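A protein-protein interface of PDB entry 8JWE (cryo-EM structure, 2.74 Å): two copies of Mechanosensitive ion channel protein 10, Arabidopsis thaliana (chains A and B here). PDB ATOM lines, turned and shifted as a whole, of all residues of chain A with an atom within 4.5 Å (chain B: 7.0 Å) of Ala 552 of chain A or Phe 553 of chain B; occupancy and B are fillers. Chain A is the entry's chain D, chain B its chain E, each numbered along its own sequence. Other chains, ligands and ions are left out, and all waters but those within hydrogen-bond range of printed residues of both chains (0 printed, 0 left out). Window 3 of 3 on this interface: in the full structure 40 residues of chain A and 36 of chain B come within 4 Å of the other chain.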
ATOM      1  N   LEU A 548      -4.648 -13.510   7.731  1.00  0.00           N
ATOM      2  CA  LEU A 548      -5.107 -14.760   8.341  1.00  0.00           C
ATOM      3  C   LEU A 548      -6.146 -14.514   9.401  1.00  0.00           C
ATOM      4  O   LEU A 548      -7.167 -15.194   9.422  1.00  0.00           O
ATOM      5  CB  LEU A 548      -3.953 -15.530   8.975  1.00  0.00           C
ATOM      6  CG  LEU A 548      -4.378 -16.656   9.955  1.00  0.00           C
ATOM      7  CD1 LEU A 548      -5.037 -17.845   9.276  1.00  0.00           C
ATOM      8  CD2 LEU A 548      -3.299 -17.094  10.907  1.00  0.00           C
ATOM      9  N   VAL A 549      -5.917 -13.538  10.256  1.00  0.00           N
ATOM     10  CA  VAL A 549      -6.926 -13.056  11.171  1.00  0.00           C
ATOM     11  C   VAL A 549      -8.034 -12.319  10.439  1.00  0.00           C
ATOM     12  O   VAL A 549      -9.161 -12.254  10.940  1.00  0.00           O
ATOM     13  CB  VAL A 549      -6.195 -12.224  12.244  1.00  0.00           C
ATOM     14  CG1 VAL A 549      -7.106 -11.443  13.162  1.00  0.00           C
ATOM     15  CG2 VAL A 549      -5.406 -13.156  13.095  1.00  0.00           C
ATOM     16  N   ALA A 550      -7.784 -11.810   9.246  1.00  0.00           N
ATOM     17  CA  ALA A 550      -8.901 -11.177   8.558  1.00  0.00           C
ATOM     18  C   ALA A 550      -9.837 -12.216   7.961  1.00  0.00           C
ATOM     19  O   ALA A 550     -11.053 -12.119   8.108  1.00  0.00           O
ATOM     20  CB  ALA A 550      -8.414 -10.211   7.481  1.00  0.00           C
ATOM     21  N   LEU A 551      -9.301 -13.279   7.383  1.00  0.00           N
ATOM     22  CA  LEU A 551     -10.186 -14.297   6.859  1.00  0.00           C
ATOM     23  C   LEU A 551     -10.801 -15.182   7.924  1.00  0.00           C
ATOM     24  O   LEU A 551     -11.377 -16.191   7.593  1.00  0.00           O
ATOM     25  CB  LEU A 551      -9.498 -15.139   5.819  1.00  0.00           C
ATOM     26  CG  LEU A 551      -8.205 -15.873   5.943  1.00  0.00           C
ATOM     27  CD1 LEU A 551      -8.292 -17.230   6.629  1.00  0.00           C
ATOM     28  CD2 LEU A 551      -7.753 -16.038   4.499  1.00  0.00           C
ATOM     29  N   ALA A 552     -10.702 -14.855   9.179  1.00  0.00           N
ATOM     30  CA  ALA A 552     -11.615 -15.468  10.105  1.00  0.00           C
ATOM     31  C   ALA A 552     -12.713 -14.525  10.560  1.00  0.00           C
ATOM     32  O   ALA A 552     -13.326 -14.795  11.585  1.00  0.00           O
ATOM     33  CB  ALA A 552     -10.850 -16.050  11.274  1.00  0.00           C
ATOM     34  N   PHE A 553     -12.974 -13.415   9.867  1.00  0.00           N
ATOM     35  CA  PHE A 553     -14.317 -12.814   9.853  1.00  0.00           C
ATOM     36  C   PHE A 553     -15.144 -13.293   8.679  1.00  0.00           C
ATOM     37  O   PHE A 553     -16.336 -13.007   8.631  1.00  0.00           O
ATOM     38  CB  PHE A 553     -14.323 -11.271   9.784  1.00  0.00           C
ATOM     39  CG  PHE A 553     -13.835 -10.601  11.022  1.00  0.00           C
ATOM     40  CD1 PHE A 553     -14.594 -10.610  12.170  1.00  0.00           C
ATOM     41  CD2 PHE A 553     -12.618  -9.929  11.034  1.00  0.00           C
ATOM     42  CE1 PHE A 553     -14.126  -9.988  13.307  1.00  0.00           C
ATOM     43  CE2 PHE A 553     -12.154  -9.311  12.159  1.00  0.00           C
ATOM     44  CZ  PHE A 553     -12.903  -9.331  13.293  1.00  0.00           C
ATOM     45  N   ILE A 554     -14.544 -13.999   7.742  1.00  0.00           N
ATOM     46  CA  ILE A 554     -15.249 -14.474   6.578  1.00  0.00           C
ATOM     47  C   ILE A 554     -15.532 -15.948   6.773  1.00  0.00           C
ATOM     48  O   ILE A 554     -16.686 -16.339   6.914  1.00  0.00           O
ATOM     49  CB  ILE A 554     -14.419 -14.210   5.325  1.00  0.00           C
ATOM     50  CG1 ILE A 554     -14.053 -12.744   5.295  1.00  0.00           C
ATOM     51  CG2 ILE A 554     -15.196 -14.532   4.104  1.00  0.00           C
ATOM     52  CD1 ILE A 554     -12.981 -12.409   4.355  1.00  0.00           C
ATOM     53  N   GLY A 556     -14.853 -17.906   9.211  1.00  0.00           N
ATOM     54  CA  GLY A 556     -14.853 -18.402  10.560  1.00  0.00           C
ATOM     55  C   GLY A 556     -16.115 -19.059  11.039  1.00  0.00           C
ATOM     56  O   GLY A 556     -16.049 -20.067  11.715  1.00  0.00           O
ATOM     57  N   LYS A 560     -16.895 -23.123  11.784  1.00  0.00           N
ATOM     58  CA  LYS A 560     -17.540 -23.503  13.011  1.00  0.00           C
ATOM     59  C   LYS A 560     -18.624 -24.515  12.766  1.00  0.00           C
ATOM     60  O   LYS A 560     -18.814 -25.408  13.570  1.00  0.00           O
ATOM     61  CB  LYS A 560     -18.127 -22.291  13.650  1.00  0.00           C
ATOM     62  CG  LYS A 560     -18.581 -22.496  14.952  1.00  0.00           C
ATOM     63  CD  LYS A 560     -18.901 -21.226  15.551  1.00  0.00           C
ATOM     64  CE  LYS A 560     -20.301 -20.867  15.301  1.00  0.00           C
ATOM     65  NZ  LYS A 560     -21.148 -21.652  16.223  1.00  0.00           N
ATOM     66  N   LEU B 548      -2.885 -21.517  17.511  1.00  0.00           N
ATOM     67  CA  LEU B 548      -3.645 -21.899  18.702  1.00  0.00           C
ATOM     68  C   LEU B 548      -4.827 -20.995  18.924  1.00  0.00           C
ATOM     69  O   LEU B 548      -5.923 -21.479  19.184  1.00  0.00           O
ATOM     70  CB  LEU B 548      -2.777 -21.865  19.956  1.00  0.00           C
ATOM     71  CG  LEU B 548      -3.562 -21.887  21.295  1.00  0.00           C
ATOM     72  CD1 LEU B 548      -4.246 -23.212  21.586  1.00  0.00           C
ATOM     73  CD2 LEU B 548      -2.780 -21.398  22.484  1.00  0.00           C
ATOM     74  N   VAL B 549      -4.628 -19.699  18.794  1.00  0.00           N
ATOM     75  CA  VAL B 549      -5.715 -18.748  18.757  1.00  0.00           C
ATOM     76  C   VAL B 549      -6.523 -18.875  17.478  1.00  0.00           C
ATOM     77  O   VAL B 549      -7.704 -18.516  17.461  1.00  0.00           O
ATOM     78  CB  VAL B 549      -5.097 -17.354  18.994  1.00  0.00           C
ATOM     79  CG1 VAL B 549      -6.044 -16.199  18.764  1.00  0.00           C
ATOM     80  CG2 VAL B 549      -4.651 -17.282  20.413  1.00  0.00           C
ATOM     81  N   ALA B 550      -5.961 -19.427  16.418  1.00  0.00           N
ATOM     82  CA  ALA B 550      -6.803 -19.591  15.240  1.00  0.00           C
ATOM     83  C   ALA B 550      -7.747 -20.772  15.402  1.00  0.00           C
ATOM     84  O   ALA B 550      -8.937 -20.662  15.119  1.00  0.00           O
ATOM     85  CB  ALA B 550      -5.962 -19.745  13.975  1.00  0.00           C
ATOM     86  N   LEU B 551      -7.276 -21.875  15.961  1.00  0.00           N
ATOM     87  CA  LEU B 551      -8.183 -22.984  16.165  1.00  0.00           C
ATOM     88  C   LEU B 551      -9.132 -22.794  17.331  1.00  0.00           C
ATOM     89  O   LEU B 551      -9.777 -23.737  17.726  1.00  0.00           O
ATOM     90  CB  LEU B 551      -7.437 -24.282  16.308  1.00  0.00           C
ATOM     91  CG  LEU B 551      -6.325 -24.601  17.253  1.00  0.00           C
ATOM     92  CD1 LEU B 551      -6.759 -24.978  18.663  1.00  0.00           C
ATOM     93  CD2 LEU B 551      -5.621 -25.773  16.584  1.00  0.00           C
ATOM     94  N   ALA B 552      -9.240 -21.629  17.898  1.00  0.00           N
ATOM     95  CA  ALA B 552     -10.406 -21.381  18.702  1.00  0.00           C
ATOM     96  C   ALA B 552     -11.414 -20.480  18.015  1.00  0.00           C
ATOM     97  O   ALA B 552     -12.257 -19.916  18.702  1.00  0.00           O
ATOM     98  CB  ALA B 552      -9.995 -20.841  20.055  1.00  0.00           C
ATOM     99  N   PHE B 553     -11.354 -20.288  16.695  1.00  0.00           N
ATOM    100  CA  PHE B 553     -12.555 -19.977  15.908  1.00  0.00           C
ATOM    101  C   PHE B 553     -13.190 -21.220  15.321  1.00  0.00           C
ATOM    102  O   PHE B 553     -14.289 -21.133  14.781  1.00  0.00           O
ATOM    103  CB  PHE B 553     -12.308 -19.017  14.722  1.00  0.00           C
ATOM    104  CG  PHE B 553     -11.984 -17.619  15.122  1.00  0.00           C
ATOM    105  CD1 PHE B 553     -12.952 -16.801  15.657  1.00  0.00           C
ATOM    106  CD2 PHE B 553     -10.705 -17.105  14.936  1.00  0.00           C
ATOM    107  CE1 PHE B 553     -12.635 -15.512  16.024  1.00  0.00           C
ATOM    108  CE2 PHE B 553     -10.390 -15.829  15.299  1.00  0.00           C
ATOM    109  CZ  PHE B 553     -11.347 -15.026  15.835  1.00  0.00           C
ATOM    110  N   ILE B 554     -12.528 -22.357  15.406  1.00  0.00           N
ATOM    111  CA  ILE B 554     -13.048 -23.582  14.855  1.00  0.00           C
ATOM    112  C   ILE B 554     -13.590 -24.416  15.996  1.00  0.00           C
ATOM    113  O   ILE B 554     -14.795 -24.628  16.085  1.00  0.00           O
ATOM    114  CB  ILE B 554     -11.950 -24.309  14.084  1.00  0.00           C
ATOM    115  CG1 ILE B 554     -11.364 -23.352  13.072  1.00  0.00           C
ATOM    116  CG2 ILE B 554     -12.503 -25.482  13.365  1.00  0.00           C
ATOM    117  CD1 ILE B 554     -10.083 -23.784  12.504  1.00  0.00           C
ATOM    118  N   ILE B 555     -12.724 -24.834  16.917  1.00  0.00           N
ATOM    119  CA  ILE B 555     -13.101 -25.805  17.923  1.00  0.00           C
ATOM    120  C   ILE B 555     -13.564 -25.111  19.180  1.00  0.00           C
ATOM    121  O   ILE B 555     -13.851 -25.752  20.176  1.00  0.00           O
ATOM    122  CB  ILE B 555     -11.965 -26.792  18.215  1.00  0.00           C
ATOM    123  CG1 ILE B 555     -10.922 -26.258  19.175  1.00  0.00           C
ATOM    124  CG2 ILE B 555     -11.277 -27.096  16.982  1.00  0.00           C
ATOM    125  CD1 ILE B 555      -9.931 -27.249  19.596  1.00  0.00           C
ATOM    126  N   GLY B 556     -13.732 -23.825  19.137  1.00  0.00           N
ATOM    127  CA  GLY B 556     -14.083 -23.133  20.347  1.00  0.00           C
ATOM    128  C   GLY B 556     -15.502 -23.269  20.817  1.00  0.00           C
ATOM    129  O   GLY B 556     -15.731 -23.418  22.002  1.00  0.00           O
ATOM    130  N   SER B 557     -16.462 -23.225  19.913  1.00  0.00           N
ATOM    131  CA  SER B 557     -17.842 -23.389  20.315  1.00  0.00           C
ATOM    132  C   SER B 557     -18.200 -24.810  20.631  1.00  0.00           C
ATOM    133  O   SER B 557     -19.255 -25.044  21.202  1.00  0.00           O
ATOM    134  CB  SER B 557     -18.787 -22.957  19.232  1.00  0.00           C
ATOM    135  OG  SER B 557     -18.768 -23.925  18.221  1.00  0.00           O
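Ala 552 of chain A touches Phe 553 of chain B, but with the chains exchanged Phe 553 of chain A does not touch Ala 552 of chain B (10.9 Å). Gly 556 of chain A touches Phe 553 of chain B, but with the chains exchanged Phe 553 of chain A does not touch Gly 556 of chain B (14.0 Å).
Among the printed residues, pairs that only touch across the chains: Lys 560 of chain A with Ser 557 of chain B (3.6 Å), Gly 556 of chain A with Phe 553 of chain B (3.7 Å) and Ala 552 of chain A with Phe 553 of chain B (3.8 Å).
Hydrophobic or aromatic side chains of chain B within 4 Å of the printed part of chain A: Phe 553. Hydrophobic or aromatic side chains of chain A that line the printed part of chain B: Ala 552. Among the printed residues, 3 pairs touch across the chains.
Of chain B, only Phe 553 (3.8 Å) comes within 4 Å of Ala 552 of chain A. Of the printed residues of chain B, Gly 556 of chain A touches Phe 553. Printed residues of chain B within 4 Å of Lys 560 of chain A: Ser 557. Of the printed residues of chain A, Phe 553 of chain B touches Ala 552 (3.8 Å) and Gly 556 (3.7 Å). Of the printed residues of chain A, Ser 557 of chain B touches Lys 560 (3.6 Å).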
